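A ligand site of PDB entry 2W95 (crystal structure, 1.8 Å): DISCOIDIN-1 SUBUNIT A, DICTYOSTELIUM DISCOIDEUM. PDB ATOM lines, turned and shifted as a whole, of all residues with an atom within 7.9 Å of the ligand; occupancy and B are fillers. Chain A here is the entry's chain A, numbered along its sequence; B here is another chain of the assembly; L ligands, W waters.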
ATOM      1  N   GLY A 179       6.362 -15.841  -9.299  1.00  0.00           N
ATOM      2  CA  GLY A 179       6.714 -16.904  -8.364  1.00  0.00           C
ATOM      3  C   GLY A 179       6.168 -18.235  -8.862  1.00  0.00           C
ATOM      4  O   GLY A 179       5.642 -18.316  -9.979  1.00  0.00           O
ATOM      5  N   LYS A 180       6.313 -19.274  -8.060  1.00  0.00           N
ATOM      6  CA  LYS A 180       5.756 -20.602  -8.408  1.00  0.00           C
ATOM      7  C   LYS A 180       4.256 -20.550  -8.562  1.00  0.00           C
ATOM      8  O   LYS A 180       3.496 -20.111  -7.653  1.00  0.00           O
ATOM      9  CB  LYS A 180       6.132 -21.627  -7.336  1.00  0.00           C
ATOM     10  CG  LYS A 180       5.710 -23.057  -7.666  1.00  0.00           C
ATOM     11  CD  LYS A 180       6.404 -24.080  -6.805  1.00  0.00           C
ATOM     12  CE  LYS A 180       6.276 -25.472  -7.459  1.00  0.00           C
ATOM     13  NZ  LYS A 180       6.268 -25.322  -8.955  1.00  0.00           N
ATOM     14  N   ALA A 211      11.782 -14.786 -19.732  1.00  0.00           N
ATOM     15  CA  ALA A 211      11.921 -13.791 -18.666  1.00  0.00           C
ATOM     16  C   ALA A 211      13.420 -13.540 -18.545  1.00  0.00           C
ATOM     17  O   ALA A 211      14.216 -14.407 -18.207  1.00  0.00           O
ATOM     18  CB  ALA A 211      11.320 -14.271 -17.355  1.00  0.00           C
ATOM     19  N   THR A 212      13.844 -12.338 -18.929  1.00  0.00           N
ATOM     20  CA  THR A 212      15.263 -12.096 -19.088  1.00  0.00           C
ATOM     21  C   THR A 212      15.950 -13.280 -19.789  1.00  0.00           C
ATOM     22  O   THR A 212      16.996 -13.792 -19.328  1.00  0.00           O
ATOM     23  CB  THR A 212      15.930 -11.757 -17.761  1.00  0.00           C
ATOM     24  OG1 THR A 212      15.147 -10.793 -17.073  1.00  0.00           O
ATOM     25  CG2 THR A 212      17.298 -11.160 -18.038  1.00  0.00           C
ATOM     26  N   GLN A 214      15.243 -16.326 -20.075  1.00  0.00           N
ATOM     27  CA  GLN A 214      15.111 -17.654 -19.520  1.00  0.00           C
ATOM     28  C   GLN A 214      13.751 -18.247 -19.825  1.00  0.00           C
ATOM     29  O   GLN A 214      12.733 -17.575 -19.606  1.00  0.00           O
ATOM     30  CB  GLN A 214      15.320 -17.621 -17.998  1.00  0.00           C
ATOM     31  CG  GLN A 214      15.858 -18.931 -17.365  1.00  0.00           C
ATOM     32  CD  GLN A 214      17.298 -19.266 -17.721  1.00  0.00           C
ATOM     33  OE1 GLN A 214      18.027 -18.445 -18.306  1.00  0.00           O
ATOM     34  NE2 GLN A 214      17.709 -20.508 -17.404  1.00  0.00           N
ATOM     35  N   THR A 215      13.735 -19.500 -20.290  1.00  0.00           N
ATOM     36  CA  THR A 215      12.517 -20.320 -20.347  1.00  0.00           C
ATOM     37  C   THR A 215      12.438 -21.143 -19.069  1.00  0.00           C
ATOM     38  O   THR A 215      13.442 -21.724 -18.663  1.00  0.00           O
ATOM     39  CB  THR A 215      12.575 -21.239 -21.579  1.00  0.00           C
ATOM     40  OG1 THR A 215      12.528 -20.437 -22.745  1.00  0.00           O
ATOM     41  CG2 THR A 215      11.384 -22.207 -21.655  1.00  0.00           C
ATOM     42  N   ARG A 216      11.276 -21.137 -18.428  1.00  0.00           N
ATOM     43  CA  ARG A 216      11.020 -21.926 -17.223  1.00  0.00           C
ATOM     44  C   ARG A 216       9.634 -22.539 -17.316  1.00  0.00           C
ATOM     45  O   ARG A 216       8.616 -21.869 -17.117  1.00  0.00           O
ATOM     46  CB  ARG A 216      11.105 -21.059 -15.956  1.00  0.00           C
ATOM     47  CG  ARG A 216      12.495 -20.474 -15.681  1.00  0.00           C
ATOM     48  CD  ARG A 216      12.455 -19.509 -14.472  1.00  0.00           C
ATOM     49  NE  ARG A 216      13.765 -18.914 -14.237  1.00  0.00           N
ATOM     50  CZ  ARG A 216      14.085 -17.657 -14.525  1.00  0.00           C
ATOM     51  NH1 ARG A 216      13.193 -16.829 -15.040  1.00  0.00           N
ATOM     52  NH2 ARG A 216      15.317 -17.233 -14.307  1.00  0.00           N
ATOM     53  N   TRP A 236       7.653 -20.619 -12.870  1.00  0.00           N
ATOM     54  CA  TRP A 236       8.176 -19.993 -11.685  1.00  0.00           C
ATOM     55  C   TRP A 236       8.927 -18.712 -12.055  1.00  0.00           C
ATOM     56  O   TRP A 236       8.902 -18.269 -13.213  1.00  0.00           O
ATOM     57  CB  TRP A 236       9.008 -20.977 -10.817  1.00  0.00           C
ATOM     58  CG  TRP A 236      10.275 -21.516 -11.407  1.00  0.00           C
ATOM     59  CD1 TRP A 236      11.550 -21.133 -11.116  1.00  0.00           C
ATOM     60  CD2 TRP A 236      10.396 -22.585 -12.357  1.00  0.00           C
ATOM     61  NE1 TRP A 236      12.454 -21.857 -11.852  1.00  0.00           N
ATOM     62  CE2 TRP A 236      11.770 -22.750 -12.626  1.00  0.00           C
ATOM     63  CE3 TRP A 236       9.480 -23.401 -13.026  1.00  0.00           C
ATOM     64  CZ2 TRP A 236      12.253 -23.713 -13.534  1.00  0.00           C
ATOM     65  CZ3 TRP A 236       9.946 -24.341 -13.936  1.00  0.00           C
ATOM     66  CH2 TRP A 236      11.304 -24.483 -14.196  1.00  0.00           C
ATOM     67  N   ASN A 237       9.507 -18.059 -11.053  1.00  0.00           N
ATOM     68  CA  ASN A 237      10.166 -16.774 -11.303  1.00  0.00           C
ATOM     69  C   ASN A 237       9.166 -15.818 -11.979  1.00  0.00           C
ATOM     70  O   ASN A 237       7.989 -15.864 -11.654  1.00  0.00           O
ATOM     71  CB  ASN A 237      11.474 -17.018 -12.077  1.00  0.00           C
ATOM     72  CG  ASN A 237      12.473 -15.851 -11.947  1.00  0.00           C
ATOM     73  OD1 ASN A 237      12.158 -14.713 -12.356  1.00  0.00           O
ATOM     74  ND2 ASN A 237      13.668 -16.129 -11.424  1.00  0.00           N
ATOM     75  N   GLU A 238       9.574 -14.941 -12.909  1.00  0.00           N
ATOM     76  CA  GLU A 238       8.624 -13.976 -13.485  1.00  0.00           C
ATOM     77  C   GLU A 238       8.041 -14.421 -14.825  1.00  0.00           C
ATOM     78  O   GLU A 238       7.376 -13.645 -15.537  1.00  0.00           O
ATOM     79  CB  GLU A 238       9.325 -12.614 -13.701  1.00  0.00           C
ATOM     80  CG  GLU A 238       9.813 -12.014 -12.404  1.00  0.00           C
ATOM     81  CD  GLU A 238       8.674 -11.653 -11.479  1.00  0.00           C
ATOM     82  OE1 GLU A 238       7.621 -11.193 -11.966  1.00  0.00           O
ATOM     83  OE2 GLU A 238       8.823 -11.826 -10.242  1.00  0.00           O
ATOM     84  N   ASN A 239       8.253 -15.691 -15.158  1.00  0.00           N
ATOM     85  CA  ASN A 239       7.805 -16.177 -16.474  1.00  0.00           C
ATOM     86  C   ASN A 239       6.308 -16.178 -16.654  1.00  0.00           C
ATOM     87  O   ASN A 239       5.540 -16.530 -15.744  1.00  0.00           O
ATOM     88  CB  ASN A 239       8.368 -17.592 -16.756  1.00  0.00           C
ATOM     89  CG  ASN A 239       9.843 -17.579 -17.008  1.00  0.00           C
ATOM     90  OD1 ASN A 239      10.622 -17.331 -16.084  1.00  0.00           O
ATOM     91  ND2 ASN A 239      10.262 -17.776 -18.266  1.00  0.00           N
ATOM     92  N   TYR B 167      17.135 -36.302 -14.154  1.00  0.00           N
ATOM     93  CA  TYR B 167      17.411 -34.853 -14.016  1.00  0.00           C
ATOM     94  C   TYR B 167      18.906 -34.521 -14.172  1.00  0.00           C
ATOM     95  O   TYR B 167      19.766 -35.233 -13.666  1.00  0.00           O
ATOM     96  CB  TYR B 167      16.909 -34.410 -12.646  1.00  0.00           C
ATOM     97  CG  TYR B 167      16.916 -32.923 -12.460  1.00  0.00           C
ATOM     98  CD1 TYR B 167      16.336 -32.078 -13.408  1.00  0.00           C
ATOM     99  CD2 TYR B 167      17.461 -32.354 -11.301  1.00  0.00           C
ATOM    100  CE1 TYR B 167      16.343 -30.663 -13.227  1.00  0.00           C
ATOM    101  CE2 TYR B 167      17.475 -30.950 -11.119  1.00  0.00           C
ATOM    102  CZ  TYR B 167      16.932 -30.131 -12.065  1.00  0.00           C
ATOM    103  OH  TYR B 167      16.941 -28.754 -11.860  1.00  0.00           O
ATOM    104  N   ASP B 170      20.487 -29.107 -10.730  1.00  0.00           N
ATOM    105  CA  ASP B 170      20.496 -27.634 -10.855  1.00  0.00           C
ATOM    106  C   ASP B 170      21.836 -27.101 -11.357  1.00  0.00           C
ATOM    107  O   ASP B 170      22.890 -27.635 -11.035  1.00  0.00           O
ATOM    108  CB  ASP B 170      20.189 -26.991  -9.500  1.00  0.00           C
ATOM    109  CG  ASP B 170      18.842 -27.378  -8.958  1.00  0.00           C
ATOM    110  OD1 ASP B 170      17.914 -27.723  -9.734  1.00  0.00           O
ATOM    111  OD2 ASP B 170      18.696 -27.309  -7.720  1.00  0.00           O
ATOM    112  N   ASN B 171      21.795 -26.049 -12.171  1.00  0.00           N
ATOM    113  CA  ASN B 171      23.014 -25.377 -12.584  1.00  0.00           C
ATOM    114  C   ASN B 171      24.067 -26.352 -13.091  1.00  0.00           C
ATOM    115  O   ASN B 171      25.253 -26.325 -12.722  1.00  0.00           O
ATOM    116  CB  ASN B 171      23.583 -24.537 -11.426  1.00  0.00           C
ATOM    117  CG  ASN B 171      24.721 -23.621 -11.878  1.00  0.00           C
ATOM    118  OD1 ASN B 171      24.840 -23.233 -13.052  1.00  0.00           O
ATOM    119  ND2 ASN B 171      25.577 -23.271 -10.923  1.00  0.00           N
ATOM    120  N   ASN B 175      25.248 -25.357 -18.344  1.00  0.00           N
ATOM    121  CA  ASN B 175      25.011 -23.932 -18.033  1.00  0.00           C
ATOM    122  C   ASN B 175      26.279 -23.060 -18.121  1.00  0.00           C
ATOM    123  O   ASN B 175      26.250 -21.904 -17.698  1.00  0.00           O
ATOM    124  CB  ASN B 175      24.437 -23.801 -16.639  1.00  0.00           C
ATOM    125  CG  ASN B 175      23.597 -22.540 -16.445  1.00  0.00           C
ATOM    126  OD1 ASN B 175      23.048 -22.005 -17.399  1.00  0.00           O
ATOM    127  ND2 ASN B 175      23.494 -22.081 -15.197  1.00  0.00           N
ATOM    128  N   GLN B 205      10.646 -30.843 -17.926  1.00  0.00           N
ATOM    129  CA  GLN B 205      10.988 -29.564 -17.223  1.00  0.00           C
ATOM    130  C   GLN B 205      12.164 -28.937 -17.924  1.00  0.00           C
ATOM    131  O   GLN B 205      13.185 -29.590 -18.144  1.00  0.00           O
ATOM    132  CB  GLN B 205      11.272 -29.760 -15.733  1.00  0.00           C
ATOM    133  CG  GLN B 205      11.243 -28.452 -14.922  1.00  0.00           C
ATOM    134  CD  GLN B 205      11.670 -28.645 -13.493  1.00  0.00           C
ATOM    135  OE1 GLN B 205      10.850 -28.695 -12.596  1.00  0.00           O
ATOM    136  NE2 GLN B 205      13.018 -28.748 -13.275  1.00  0.00           N
ATOM    137  N   ILE B 206      12.010 -27.671 -18.303  1.00  0.00           N
ATOM    138  CA  ILE B 206      13.019 -27.016 -19.116  1.00  0.00           C
ATOM    139  C   ILE B 206      13.382 -25.671 -18.438  1.00  0.00           C
ATOM    140  O   ILE B 206      12.491 -24.900 -18.116  1.00  0.00           O
ATOM    141  CB  ILE B 206      12.480 -26.763 -20.539  1.00  0.00           C
ATOM    142  CG1 ILE B 206      12.408 -28.074 -21.341  1.00  0.00           C
ATOM    143  CG2 ILE B 206      13.369 -25.787 -21.277  1.00  0.00           C
ATOM    144  CD1 ILE B 206      11.618 -28.040 -22.587  1.00  0.00           C
ATOM    145  N   ASP B 207      14.658 -25.474 -18.172  1.00  0.00           N
ATOM    146  CA  ASP B 207      15.184 -24.249 -17.515  1.00  0.00           C
ATOM    147  C   ASP B 207      16.445 -23.844 -18.269  1.00  0.00           C
ATOM    148  O   ASP B 207      17.542 -24.374 -18.057  1.00  0.00           O
ATOM    149  CB  ASP B 207      15.409 -24.558 -16.037  1.00  0.00           C
ATOM    150  CG  ASP B 207      15.674 -23.305 -15.181  1.00  0.00           C
ATOM    151  OD1 ASP B 207      15.884 -22.183 -15.729  1.00  0.00           O
ATOM    152  OD2 ASP B 207      15.639 -23.489 -13.963  1.00  0.00           O
ATOM    153  N   CYS B 208      16.273 -22.924 -19.223  1.00  0.00           N
ATOM    154  CA  CYS B 208      17.358 -22.616 -20.159  1.00  0.00           C
ATOM    155  C   CYS B 208      17.328 -21.164 -20.643  1.00  0.00           C
ATOM    156  O   CYS B 208      16.281 -20.503 -20.624  1.00  0.00           O
ATOM    157  CB  CYS B 208      17.318 -23.575 -21.339  1.00  0.00           C
ATOM    158  SG  CYS B 208      15.854 -23.492 -22.328  1.00  0.00           S
ATOM    159  N   THR B 209      18.494 -20.700 -21.090  1.00  0.00           N
ATOM    160  CA  THR B 209      18.674 -19.321 -21.548  1.00  0.00           C
ATOM    161  C   THR B 209      18.843 -19.333 -23.042  1.00  0.00           C
ATOM    162  O   THR B 209      19.612 -20.120 -23.573  1.00  0.00           O
ATOM    163  CB  THR B 209      19.986 -18.691 -20.996  1.00  0.00           C
ATOM    164  OG1 THR B 209      20.091 -18.936 -19.602  1.00  0.00           O
ATOM    165  CG2 THR B 209      20.000 -17.197 -21.232  1.00  0.00           C
ATOM    166  N   LYS B 240      23.311 -21.617 -22.846  1.00  0.00           N
ATOM    167  CA  LYS B 240      23.480 -21.962 -21.435  1.00  0.00           C
ATOM    168  C   LYS B 240      22.167 -22.582 -20.935  1.00  0.00           C
ATOM    169  O   LYS B 240      21.093 -21.967 -21.043  1.00  0.00           O
ATOM    170  CB  LYS B 240      23.834 -20.726 -20.608  1.00  0.00           C
ATOM    171  CG  LYS B 240      25.045 -19.932 -21.161  1.00  0.00           C
ATOM    172  CD  LYS B 240      26.334 -20.716 -21.070  1.00  0.00           C
ATOM    173  CE  LYS B 240      27.565 -19.924 -21.623  1.00  0.00           C
ATOM    174  NZ  LYS B 240      27.810 -20.149 -23.090  1.00  0.00           N
ATOM    175  N   VAL B 241      22.248 -23.784 -20.411  1.00  0.00           N
ATOM    176  CA  VAL B 241      21.051 -24.497 -19.954  1.00  0.00           C
ATOM    177  C   VAL B 241      21.275 -24.877 -18.480  1.00  0.00           C
ATOM    178  O   VAL B 241      22.191 -25.633 -18.161  1.00  0.00           O
ATOM    179  CB  VAL B 241      20.776 -25.750 -20.830  1.00  0.00           C
ATOM    180  CG1 VAL B 241      19.589 -26.591 -20.293  1.00  0.00           C
ATOM    181  CG2 VAL B 241      20.499 -25.326 -22.237  1.00  0.00           C
ATOM    182  N   TYR B 242      20.420 -24.335 -17.620  1.00  0.00           N
ATOM    183  CA  TYR B 242      20.563 -24.471 -16.185  1.00  0.00           C
ATOM    184  C   TYR B 242      20.174 -25.890 -15.784  1.00  0.00           C
ATOM    185  O   TYR B 242      20.889 -26.538 -15.022  1.00  0.00           O
ATOM    186  CB  TYR B 242      19.677 -23.449 -15.502  1.00  0.00           C
ATOM    187  CG  TYR B 242      19.606 -23.525 -14.011  1.00  0.00           C
ATOM    188  CD1 TYR B 242      20.429 -22.703 -13.202  1.00  0.00           C
ATOM    189  CD2 TYR B 242      18.711 -24.365 -13.374  1.00  0.00           C
ATOM    190  CE1 TYR B 242      20.352 -22.756 -11.814  1.00  0.00           C
ATOM    191  CE2 TYR B 242      18.624 -24.417 -11.996  1.00  0.00           C
ATOM    192  CZ  TYR B 242      19.456 -23.609 -11.216  1.00  0.00           C
ATOM    193  OH  TYR B 242      19.346 -23.678  -9.847  1.00  0.00           O
ATOM    194  N   SER B 243      19.075 -26.394 -16.357  1.00  0.00           N
ATOM    195  CA  SER B 243      18.683 -27.781 -16.068  1.00  0.00           C
ATOM    196  C   SER B 243      17.734 -28.334 -17.089  1.00  0.00           C
ATOM    197  O   SER B 243      17.056 -27.573 -17.749  1.00  0.00           O
ATOM    198  CB  SER B 243      18.090 -27.890 -14.666  1.00  0.00           C
ATOM    199  OG  SER B 243      16.837 -27.240 -14.566  1.00  0.00           O
HETATM  200  C1  LIG L   1      16.974 -18.626 -11.060  1.00  0.00           C
HETATM  201  C2  LIG L   1      15.878 -19.697 -11.078  1.00  0.00           C
HETATM  202  C3  LIG L   1      16.436 -20.976 -11.711  1.00  0.00           C
HETATM  203  C4  LIG L   1      17.096 -20.702 -13.066  1.00  0.00           C
HETATM  204  C5  LIG L   1      18.149 -19.582 -12.912  1.00  0.00           C
HETATM  205  C6  LIG L   1      18.752 -19.217 -14.265  1.00  0.00           C
HETATM  206  C7  LIG L   1      14.284 -19.383  -9.226  1.00  0.00           C
HETATM  207  C8  LIG L   1      14.062 -19.703  -7.787  1.00  0.00           C
HETATM  208  N1  LIG L   1      15.397 -19.931  -9.735  1.00  0.00           N
HETATM  209  O1  LIG L   1      16.333 -17.428 -10.601  1.00  0.00           O
HETATM  210  O2  LIG L   1      15.357 -21.889 -11.871  1.00  0.00           O
HETATM  211  O3  LIG L   1      16.089 -20.304 -14.009  1.00  0.00           O
HETATM  212  O4  LIG L   1      17.486 -18.445 -12.368  1.00  0.00           O
HETATM  213  O5  LIG L   1      19.910 -18.377 -14.079  1.00  0.00           O
HETATM  214  O6  LIG L   1      13.482 -18.699  -9.841  1.00  0.00           O
HETATM  215  O   HOH W   1      11.969 -17.217  -8.090  1.00  0.00           O
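Merely in contact with the ligand: Gln 214 (3.6 Å) and Tyr 242 of chain B (3.9 Å). Hydrophobic or aromatic side chains within 4 Å of the ligand: Trp 236 and Tyr 242 of chain B. Six residues have an atom within 4 Å of the ligand: Gln 214, Arg 216, Trp 236, Asn 237, Asp 207 of chain B and Tyr 242 of chain B.
The side-chain carboxylate (OD1) of Asp 207 of chain B sits at hydrogen-bond distance from an oxygen (O3) of the ligand. The guanidinium group of Arg 216 sits at hydrogen-bond distance from an oxygen (O3) of the ligand, 2.7 Å away. The indole nitrogen (NE1) of Trp 236 is in hydrogen-bond range of an oxygen (O2) of the ligand (2.9 Å). The side-chain amide nitrogen (ND2) of Asn 237 lies within hydrogen-bond range of an oxygen (O6) of the ligand (3.0 Å).
NE2 of Gln 214 lies within hydrogen-bond range of OD1 of Asp 207 of chain B (3.0 Å). The backbone carbonyl oxygen of Asp 207 of chain B is in hydrogen-bond range of the backbone NH of Tyr 242 of chain B (2.9 Å). The backbone NH (N) of Ser 243 of chain B lies within hydrogen-bond range of the backbone carbonyl oxygen (O) of Asp 207 of chain B. O of Trp 236 lies close to OD1 of Asn 239, at 3.5 Å. O of Asn 237 is in hydrogen-bond range of N of Gly 179 (2.9 Å). The side-chain amide oxygen of Gln 214 is in hydrogen-bond range of the side-chain hydroxyl of Thr 209 of chain B (2.5 Å). N of Cys 208 of chain B lies close to NE2 of Gln 214. The backbone carbonyl oxygen of Gln 214 lies within hydrogen-bond range of the side-chain amide nitrogen of Asn 239.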
